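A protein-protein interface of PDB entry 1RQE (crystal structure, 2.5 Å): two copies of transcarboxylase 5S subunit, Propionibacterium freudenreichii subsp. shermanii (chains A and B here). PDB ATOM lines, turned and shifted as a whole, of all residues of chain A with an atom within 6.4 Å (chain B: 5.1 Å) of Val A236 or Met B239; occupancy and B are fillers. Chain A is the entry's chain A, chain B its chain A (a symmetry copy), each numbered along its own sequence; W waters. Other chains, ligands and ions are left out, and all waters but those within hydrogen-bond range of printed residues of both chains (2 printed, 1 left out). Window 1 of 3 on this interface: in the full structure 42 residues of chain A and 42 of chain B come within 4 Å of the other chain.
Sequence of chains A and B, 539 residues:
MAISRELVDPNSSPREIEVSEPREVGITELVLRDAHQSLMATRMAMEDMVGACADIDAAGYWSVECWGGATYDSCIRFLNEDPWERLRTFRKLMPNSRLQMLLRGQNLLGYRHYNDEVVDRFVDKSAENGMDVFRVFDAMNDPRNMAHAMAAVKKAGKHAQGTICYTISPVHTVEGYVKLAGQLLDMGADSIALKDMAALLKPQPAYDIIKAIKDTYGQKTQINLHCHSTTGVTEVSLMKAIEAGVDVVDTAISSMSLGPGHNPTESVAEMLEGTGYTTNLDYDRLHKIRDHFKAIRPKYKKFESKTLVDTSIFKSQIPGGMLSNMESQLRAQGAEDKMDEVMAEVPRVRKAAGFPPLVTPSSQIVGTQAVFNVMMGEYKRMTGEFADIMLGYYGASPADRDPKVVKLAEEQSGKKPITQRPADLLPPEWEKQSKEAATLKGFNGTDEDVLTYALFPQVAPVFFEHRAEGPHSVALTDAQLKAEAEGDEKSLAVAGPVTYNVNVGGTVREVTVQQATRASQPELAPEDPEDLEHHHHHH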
ATOM      1  N   LYS A 202       7.318  -0.302 -34.954  1.00  0.00           N
ATOM      2  CA  LYS A 202       7.333   0.842 -34.075  1.00  0.00           C
ATOM      3  C   LYS A 202       8.180   0.525 -32.854  1.00  0.00           C
ATOM      4  O   LYS A 202       8.535  -0.628 -32.616  1.00  0.00           O
ATOM      5  CB  LYS A 202       5.902   1.239 -33.707  1.00  0.00           C
ATOM      6  CG  LYS A 202       5.209   1.968 -34.865  1.00  0.00           C
ATOM      7  CD  LYS A 202       3.858   2.555 -34.481  1.00  0.00           C
ATOM      8  CE  LYS A 202       3.318   3.434 -35.597  1.00  0.00           C
ATOM      9  NZ  LYS A 202       2.044   4.088 -35.229  1.00  0.00           N
ATOM     10  N   PRO A 203       8.564   1.557 -32.094  1.00  0.00           N
ATOM     11  CA  PRO A 203       9.389   1.413 -30.886  1.00  0.00           C
ATOM     12  C   PRO A 203       8.881   0.436 -29.829  1.00  0.00           C
ATOM     13  O   PRO A 203       9.595  -0.484 -29.441  1.00  0.00           O
ATOM     14  CB  PRO A 203       9.472   2.836 -30.360  1.00  0.00           C
ATOM     15  CG  PRO A 203       9.500   3.635 -31.617  1.00  0.00           C
ATOM     16  CD  PRO A 203       8.432   2.977 -32.473  1.00  0.00           C
ATOM     17  N   ALA A 206       8.832  -3.122 -31.012  1.00  0.00           N
ATOM     18  CA  ALA A 206      10.192  -3.607 -31.170  1.00  0.00           C
ATOM     19  C   ALA A 206      10.692  -4.126 -29.832  1.00  0.00           C
ATOM     20  O   ALA A 206      11.286  -5.203 -29.742  1.00  0.00           O
ATOM     21  CB  ALA A 206      11.096  -2.491 -31.681  1.00  0.00           C
ATOM     22  N   GLY A 232      10.372   6.737 -41.068  1.00  0.00           N
ATOM     23  CA  GLY A 232      10.999   7.696 -40.183  1.00  0.00           C
ATOM     24  C   GLY A 232      10.986   7.406 -38.699  1.00  0.00           C
ATOM     25  O   GLY A 232      11.486   8.227 -37.930  1.00  0.00           O
ATOM     26  N   VAL A 233      10.446   6.256 -38.286  1.00  0.00           N
ATOM     27  CA  VAL A 233      10.374   5.911 -36.861  1.00  0.00           C
ATOM     28  C   VAL A 233      11.294   4.773 -36.420  1.00  0.00           C
ATOM     29  O   VAL A 233      11.418   4.504 -35.222  1.00  0.00           O
ATOM     30  CB  VAL A 233       8.929   5.472 -36.440  1.00  0.00           C
ATOM     31  CG1 VAL A 233       7.877   6.360 -37.095  1.00  0.00           C
ATOM     32  CG2 VAL A 233       8.689   3.993 -36.801  1.00  0.00           C
ATOM     33  N   THR A 234      11.940   4.101 -37.362  1.00  0.00           N
ATOM     34  CA  THR A 234      12.753   2.945 -37.005  1.00  0.00           C
ATOM     35  C   THR A 234      14.055   3.143 -36.245  1.00  0.00           C
ATOM     36  O   THR A 234      14.533   2.203 -35.599  1.00  0.00           O
ATOM     37  CB  THR A 234      13.033   2.057 -38.235  1.00  0.00           C
ATOM     38  OG1 THR A 234      13.712   2.818 -39.247  1.00  0.00           O
ATOM     39  CG2 THR A 234      11.725   1.501 -38.784  1.00  0.00           C
ATOM     40  N   GLU A 235      14.656   4.327 -36.305  1.00  0.00           N
ATOM     41  CA  GLU A 235      15.872   4.478 -35.536  1.00  0.00           C
ATOM     42  C   GLU A 235      15.518   4.486 -34.047  1.00  0.00           C
ATOM     43  O   GLU A 235      16.302   4.051 -33.208  1.00  0.00           O
ATOM     44  CB  GLU A 235      16.623   5.746 -35.893  1.00  0.00           C
ATOM     45  CG  GLU A 235      17.942   5.796 -35.148  1.00  0.00           C
ATOM     46  CD  GLU A 235      18.928   6.750 -35.748  1.00  0.00           C
ATOM     47  OE1 GLU A 235      19.247   6.614 -36.947  1.00  0.00           O
ATOM     48  OE2 GLU A 235      19.392   7.635 -35.013  1.00  0.00           O
ATOM     49  N   VAL A 236      14.326   4.967 -33.718  1.00  0.00           N
ATOM     50  CA  VAL A 236      13.915   4.985 -32.325  1.00  0.00           C
ATOM     51  C   VAL A 236      13.609   3.545 -31.939  1.00  0.00           C
ATOM     52  O   VAL A 236      13.814   3.145 -30.798  1.00  0.00           O
ATOM     53  CB  VAL A 236      12.675   5.893 -32.112  1.00  0.00           C
ATOM     54  CG1 VAL A 236      12.283   5.923 -30.647  1.00  0.00           C
ATOM     55  CG2 VAL A 236      12.989   7.294 -32.564  1.00  0.00           C
ATOM     56  N   SER A 237      13.139   2.759 -32.906  1.00  0.00           N
ATOM     57  CA  SER A 237      12.832   1.344 -32.662  1.00  0.00           C
ATOM     58  C   SER A 237      14.129   0.570 -32.402  1.00  0.00           C
ATOM     59  O   SER A 237      14.151  -0.364 -31.612  1.00  0.00           O
ATOM     60  CB  SER A 237      12.092   0.726 -33.858  1.00  0.00           C
ATOM     61  OG  SER A 237      10.885   1.419 -34.123  1.00  0.00           O
ATOM     62  N   LEU A 238      15.207   0.958 -33.075  1.00  0.00           N
ATOM     63  CA  LEU A 238      16.491   0.305 -32.863  1.00  0.00           C
ATOM     64  C   LEU A 238      16.886   0.507 -31.411  1.00  0.00           C
ATOM     65  O   LEU A 238      17.271  -0.441 -30.729  1.00  0.00           O
ATOM     66  CB  LEU A 238      17.558   0.902 -33.777  1.00  0.00           C
ATOM     67  CG  LEU A 238      17.897   0.119 -35.041  1.00  0.00           C
ATOM     68  CD1 LEU A 238      16.644  -0.227 -35.807  1.00  0.00           C
ATOM     69  CD2 LEU A 238      18.840   0.944 -35.898  1.00  0.00           C
ATOM     70  N   MET A 239      16.778   1.742 -30.926  1.00  0.00           N
ATOM     71  CA  MET A 239      17.119   2.013 -29.538  1.00  0.00           C
ATOM     72  C   MET A 239      16.299   1.112 -28.606  1.00  0.00           C
ATOM     73  O   MET A 239      16.845   0.450 -27.722  1.00  0.00           O
ATOM     74  CB  MET A 239      16.851   3.477 -29.189  1.00  0.00           C
ATOM     75  CG  MET A 239      17.340   3.890 -27.794  1.00  0.00           C
ATOM     76  SD  MET A 239      19.147   3.970 -27.643  1.00  0.00           S
ATOM     77  CE  MET A 239      19.491   2.629 -26.553  1.00  0.00           C
ATOM     78  N   LYS A 240      14.988   1.082 -28.798  1.00  0.00           N
ATOM     79  CA  LYS A 240      14.162   0.249 -27.941  1.00  0.00           C
ATOM     80  C   LYS A 240      14.540  -1.215 -28.057  1.00  0.00           C
ATOM     81  O   LYS A 240      14.519  -1.943 -27.063  1.00  0.00           O
ATOM     82  CB  LYS A 240      12.680   0.436 -28.264  1.00  0.00           C
ATOM     83  CG  LYS A 240      12.133   1.771 -27.790  1.00  0.00           C
ATOM     84  CD  LYS A 240      12.258   1.895 -26.290  1.00  0.00           C
ATOM     85  CE  LYS A 240      12.234   3.349 -25.863  1.00  0.00           C
ATOM     86  NZ  LYS A 240      12.553   3.473 -24.417  1.00  0.00           N
ATOM     87  N   ALA A 241      14.883  -1.653 -29.264  1.00  0.00           N
ATOM     88  CA  ALA A 241      15.276  -3.039 -29.454  1.00  0.00           C
ATOM     89  C   ALA A 241      16.564  -3.285 -28.674  1.00  0.00           C
ATOM     90  O   ALA A 241      16.724  -4.328 -28.042  1.00  0.00           O
ATOM     91  CB  ALA A 241      15.483  -3.341 -30.928  1.00  0.00           C
ATOM     92  N   ASN A 263      18.618   3.205 -41.546  1.00  0.00           N
ATOM     93  CA  ASN A 263      19.143   4.190 -40.610  1.00  0.00           C
ATOM     94  C   ASN A 263      20.661   4.241 -40.797  1.00  0.00           C
ATOM     95  O   ASN A 263      21.288   3.239 -41.156  1.00  0.00           O
ATOM     96  CB  ASN A 263      18.773   3.820 -39.171  1.00  0.00           C
ATOM     97  CG  ASN A 263      17.276   3.860 -38.934  1.00  0.00           C
ATOM     98  OD1 ASN A 263      16.647   2.836 -38.673  1.00  0.00           O
ATOM     99  ND2 ASN A 263      16.695   5.045 -39.037  1.00  0.00           N
ATOM    100  N   MET A 271      24.614   7.693 -31.357  1.00  0.00           N
ATOM    101  CA  MET A 271      23.500   7.886 -30.441  1.00  0.00           C
ATOM    102  C   MET A 271      23.596   7.120 -29.128  1.00  0.00           C
ATOM    103  O   MET A 271      22.881   7.455 -28.179  1.00  0.00           O
ATOM    104  CB  MET A 271      22.189   7.525 -31.129  1.00  0.00           C
ATOM    105  CG  MET A 271      21.923   6.027 -31.182  1.00  0.00           C
ATOM    106  SD  MET A 271      20.490   5.603 -32.173  1.00  0.00           S
ATOM    107  CE  MET A 271      20.240   3.890 -31.735  1.00  0.00           C
ATOM    108  N   GLU B 235      16.164  12.138 -33.333  1.00  0.00           N
ATOM    109  CA  GLU B 235      14.826  11.635 -33.114  1.00  0.00           C
ATOM    110  C   GLU B 235      14.846  10.672 -31.925  1.00  0.00           C
ATOM    111  O   GLU B 235      13.867  10.547 -31.195  1.00  0.00           O
ATOM    112  CB  GLU B 235      14.271  10.930 -34.337  1.00  0.00           C
ATOM    113  CG  GLU B 235      12.829  10.529 -34.096  1.00  0.00           C
ATOM    114  CD  GLU B 235      12.074  10.238 -35.357  1.00  0.00           C
ATOM    115  OE1 GLU B 235      12.014  11.117 -36.241  1.00  0.00           O
ATOM    116  OE2 GLU B 235      11.531   9.127 -35.459  1.00  0.00           O
ATOM    117  N   VAL B 236      15.972  10.000 -31.719  1.00  0.00           N
ATOM    118  CA  VAL B 236      16.070   9.085 -30.596  1.00  0.00           C
ATOM    119  C   VAL B 236      16.171   9.940 -29.341  1.00  0.00           C
ATOM    120  O   VAL B 236      15.693   9.555 -28.279  1.00  0.00           O
ATOM    121  CB  VAL B 236      17.300   8.150 -30.732  1.00  0.00           C
ATOM    122  CG1 VAL B 236      17.365   7.181 -29.566  1.00  0.00           C
ATOM    123  CG2 VAL B 236      17.202   7.367 -32.014  1.00  0.00           C
ATOM    124  N   SER B 237      16.778  11.119 -29.473  1.00  0.00           N
ATOM    125  CA  SER B 237      16.914  12.043 -28.341  1.00  0.00           C
ATOM    126  C   SER B 237      15.536  12.582 -27.945  1.00  0.00           C
ATOM    127  O   SER B 237      15.271  12.818 -26.773  1.00  0.00           O
ATOM    128  CB  SER B 237      17.847  13.212 -28.692  1.00  0.00           C
ATOM    129  OG  SER B 237      19.132  12.745 -29.061  1.00  0.00           O
ATOM    130  N   LEU B 238      14.663  12.785 -28.927  1.00  0.00           N
ATOM    131  CA  LEU B 238      13.317  13.259 -28.639  1.00  0.00           C
ATOM    132  C   LEU B 238      12.633  12.227 -27.762  1.00  0.00           C
ATOM    133  O   LEU B 238      12.037  12.568 -26.742  1.00  0.00           O
ATOM    134  CB  LEU B 238      12.524  13.448 -29.930  1.00  0.00           C
ATOM    135  CG  LEU B 238      12.409  14.872 -30.464  1.00  0.00           C
ATOM    136  CD1 LEU B 238      13.768  15.522 -30.550  1.00  0.00           C
ATOM    137  CD2 LEU B 238      11.742  14.839 -31.827  1.00  0.00           C
ATOM    138  N   MET B 239      12.729  10.955 -28.145  1.00  0.00           N
ATOM    139  CA  MET B 239      12.115   9.905 -27.346  1.00  0.00           C
ATOM    140  C   MET B 239      12.640   9.960 -25.906  1.00  0.00           C
ATOM    141  O   MET B 239      11.866   9.966 -24.948  1.00  0.00           O
ATOM    142  CB  MET B 239      12.414   8.529 -27.940  1.00  0.00           C
ATOM    143  CG  MET B 239      11.667   7.374 -27.257  1.00  0.00           C
ATOM    144  SD  MET B 239       9.882   7.359 -27.587  1.00  0.00           S
ATOM    145  CE  MET B 239       9.206   7.747 -26.007  1.00  0.00           C
ATOM    146  N   LYS B 240      13.955  10.002 -25.746  1.00  0.00           N
ATOM    147  CA  LYS B 240      14.508  10.051 -24.404  1.00  0.00           C
ATOM    148  C   LYS B 240      14.052  11.291 -23.659  1.00  0.00           C
ATOM    149  O   LYS B 240      13.800  11.235 -22.455  1.00  0.00           O
ATOM    150  CB  LYS B 240      16.035   9.992 -24.440  1.00  0.00           C
ATOM    151  CG  LYS B 240      16.567   8.616 -24.798  1.00  0.00           C
ATOM    152  CD  LYS B 240      16.129   7.594 -23.777  1.00  0.00           C
ATOM    153  CE  LYS B 240      16.173   6.194 -24.359  1.00  0.00           C
ATOM    154  NZ  LYS B 240      15.557   5.220 -23.421  1.00  0.00           N
ATOM    155  N   ALA B 241      13.947  12.411 -24.367  1.00  0.00           N
ATOM    156  CA  ALA B 241      13.498  13.637 -23.730  1.00  0.00           C
ATOM    157  C   ALA B 241      12.056  13.442 -23.271  1.00  0.00           C
ATOM    158  O   ALA B 241      11.683  13.871 -22.181  1.00  0.00           O
ATOM    159  CB  ALA B 241      13.595  14.809 -24.693  1.00  0.00           C
ATOM    160  N   ILE B 242      11.243  12.790 -24.093  1.00  0.00           N
ATOM    161  CA  ILE B 242       9.862  12.551 -23.699  1.00  0.00           C
ATOM    162  C   ILE B 242       9.781  11.621 -22.488  1.00  0.00           C
ATOM    163  O   ILE B 242       8.902  11.774 -21.653  1.00  0.00           O
ATOM    164  CB  ILE B 242       9.025  11.997 -24.859  1.00  0.00           C
ATOM    165  CG1 ILE B 242       8.618  13.155 -25.770  1.00  0.00           C
ATOM    166  CG2 ILE B 242       7.779  11.290 -24.332  1.00  0.00           C
ATOM    167  CD1 ILE B 242       8.237  12.741 -27.173  1.00  0.00           C
ATOM    168  N   GLU B 243      10.703  10.675 -22.380  1.00  0.00           N
ATOM    169  CA  GLU B 243      10.704   9.777 -21.230  1.00  0.00           C
ATOM    170  C   GLU B 243      11.172  10.551 -19.994  1.00  0.00           C
ATOM    171  O   GLU B 243      10.797  10.224 -18.867  1.00  0.00           O
ATOM    172  CB  GLU B 243      11.627   8.580 -21.474  1.00  0.00           C
ATOM    173  CG  GLU B 243      11.255   7.760 -22.692  1.00  0.00           C
ATOM    174  CD  GLU B 243      12.238   6.643 -22.963  1.00  0.00           C
ATOM    175  OE1 GLU B 243      13.465   6.861 -22.806  1.00  0.00           O
ATOM    176  OE2 GLU B 243      11.782   5.548 -23.344  1.00  0.00           O
ATOM    177  N   ALA B 244      11.989  11.579 -20.214  1.00  0.00           N
ATOM    178  CA  ALA B 244      12.495  12.404 -19.122  1.00  0.00           C
ATOM    179  C   ALA B 244      11.442  13.416 -18.712  1.00  0.00           C
ATOM    180  O   ALA B 244      11.636  14.188 -17.778  1.00  0.00           O
ATOM    181  CB  ALA B 244      13.761  13.116 -19.546  1.00  0.00           C
ATOM    182  N   MET B 271       5.660   7.206 -33.887  1.00  0.00           N
ATOM    183  CA  MET B 271       6.559   6.398 -33.078  1.00  0.00           C
ATOM    184  C   MET B 271       6.121   6.181 -31.635  1.00  0.00           C
ATOM    185  O   MET B 271       6.636   5.272 -30.977  1.00  0.00           O
ATOM    186  CB  MET B 271       7.957   7.006 -33.083  1.00  0.00           C
ATOM    187  CG  MET B 271       8.111   8.183 -32.130  1.00  0.00           C
ATOM    188  SD  MET B 271       9.688   9.020 -32.298  1.00  0.00           S
ATOM    189  CE  MET B 271       9.703  10.059 -30.845  1.00  0.00           C
ATOM    190  N   LEU B 272       5.175   6.991 -31.150  1.00  0.00           N
ATOM    191  CA  LEU B 272       4.701   6.887 -29.760  1.00  0.00           C
ATOM    192  C   LEU B 272       3.641   5.820 -29.473  1.00  0.00           C
ATOM    193  O   LEU B 272       3.417   5.461 -28.314  1.00  0.00           O
ATOM    194  CB  LEU B 272       4.145   8.236 -29.273  1.00  0.00           C
ATOM    195  CG  LEU B 272       5.074   9.448 -29.277  1.00  0.00           C
ATOM    196  CD1 LEU B 272       4.299  10.695 -28.850  1.00  0.00           C
ATOM    197  CD2 LEU B 272       6.267   9.181 -28.356  1.00  0.00           C
ATOM    198  N   THR B 275       3.362   3.476 -26.235  1.00  0.00           N
ATOM    199  CA  THR B 275       4.359   3.825 -25.233  1.00  0.00           C
ATOM    200  C   THR B 275       3.719   4.419 -23.997  1.00  0.00           C
ATOM    201  O   THR B 275       4.339   4.484 -22.941  1.00  0.00           O
ATOM    202  CB  THR B 275       5.357   4.853 -25.789  1.00  0.00           C
ATOM    203  OG1 THR B 275       4.662   6.069 -26.123  1.00  0.00           O
ATOM    204  CG2 THR B 275       6.037   4.302 -27.035  1.00  0.00           C
ATOM    205  N   TYR B 277       2.676   7.401 -24.164  1.00  0.00           N
ATOM    206  CA  TYR B 277       2.708   8.800 -24.572  1.00  0.00           C
ATOM    207  C   TYR B 277       1.938   8.927 -25.877  1.00  0.00           C
ATOM    208  O   TYR B 277       1.827   7.967 -26.636  1.00  0.00           O
ATOM    209  CB  TYR B 277       4.137   9.268 -24.799  1.00  0.00           C
ATOM    210  CG  TYR B 277       5.036   9.008 -23.633  1.00  0.00           C
ATOM    211  CD1 TYR B 277       6.022   8.030 -23.708  1.00  0.00           C
ATOM    212  CD2 TYR B 277       4.913   9.745 -22.452  1.00  0.00           C
ATOM    213  CE1 TYR B 277       6.867   7.785 -22.648  1.00  0.00           C
ATOM    214  CE2 TYR B 277       5.758   9.513 -21.379  1.00  0.00           C
ATOM    215  CZ  TYR B 277       6.735   8.528 -21.488  1.00  0.00           C
ATOM    216  OH  TYR B 277       7.577   8.265 -20.444  1.00  0.00           O
HETATM  217  O   HOH W   1      17.060  10.057 -35.043  1.00  0.00           O
HETATM  218  O   HOH W   2      13.995   7.082 -36.484  1.00  0.00           O
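O of Gly A232 lies close to OE2 of Glu B235 (2.6 Å).
The side-chain carboxylate (OE2) of Glu B243 is in salt-bridge range of the side-chain amino group (NZ) of Lys A240.
The backbone carbonyl oxygen (O) of Val A233 lies within hydrogen-bond range of the side-chain hydroxyl (OG) of Ser A237 (3.3 Å).
The backbone NH of Glu A235 sits at hydrogen-bond distance from the side-chain amide oxygen of Asn A263, at 3.4 Å.
The side-chain amino group (NZ) of Lys B240 is in salt-bridge range of the side-chain carboxylate (OE1) of Glu B243, at 2.7 Å.
Among the printed residues, pairs that only touch across the chains: Pro A203 with Met B271, Val A233 with Glu B235, Val A233 with Met B271, Glu A235 with Val B236, Val A236 with Glu B235, Val A236 with Met B239, Val A236 with Met B271, Met A239 with Val B236, Lys A240 with Lys B240 and Met A271 with Val B236.
Lys A202 touches none of the printed residues of chain B.
Of chain B, only Glu B235 (3.6 Å), Met B239 (3.7 Å) and Met B271 (3.7 Å) come within 4 Å of Val A236.
Of the printed residues of chain B, Met A239 touches Val B236.
Of the printed residues of chain A, Glu B235 touches Gly A232, Val A233 and Val A236.
Of chain A, only Val A236 (3.7 Å) comes within 4 Å of Met B239.
Of the printed residues of chain A, Lys B240 touches Lys A240.
Of the printed residues of chain A, Glu B243 touches Lys A240 (2.5 Å).
Printed residues of chain A within 4 Å of Met B271: Pro A203 (3.3 Å), Val A233 (3.8 Å) and Val A236 (3.7 Å).
The nearest residue of chain A that does not touch Met B239 is Lys A240 (4.3 Å).
Printed residues of chain A that touch a printed residue of chain B: Pro A203, Gly A232, Val A233, Glu A235, Val A236, Met A239, Lys A240 and Met A271.
Hydrophobic or aromatic side chains of chain B within 4 Å of the printed part of chain A: Val B236, Met B239 and Met B271.
Along chain B the printed residues that touch a printed residue of chain A span positions 235 to 271.
Among the printed residues, Asp or Glu carboxylates within 4 Å of a Lys or Arg side-chain nitrogen of the other chain: Lys A240 with Glu B243 (2.5 Å).
Glu A235 touches Val B236, and with the chains exchanged Val A236 touches Glu B235.
Val A236 touches Met B239, and with the chains exchanged Met A239 touches Val B236.
Val A236 touches Met B271, and with the chains exchanged Met A271 touches Val B236.
Lys A240 touches its own counterpart, Lys B240.
8 positions are printed for both chains.
Of the 12 pairs that touch across the chains among the printed residues, 7 have their exchanged pair printed and touching as well.
Water W1 lies within hydrogen-bond range of N of Glu B235 (2.8 Å), OE2 of Glu A235 (3.4 Å) and N of Val B236 (3.5 Å).
Water W2 lies within hydrogen-bond range of the backbone NH (N) of Glu A235 (2.8 Å), the backbone carbonyl oxygen (O) of Gly A232 (3.1 Å), the side-chain carboxylate (OE2) of Glu B235 (3.4 Å) and the backbone NH (N) of Val A236 (3.5 Å).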
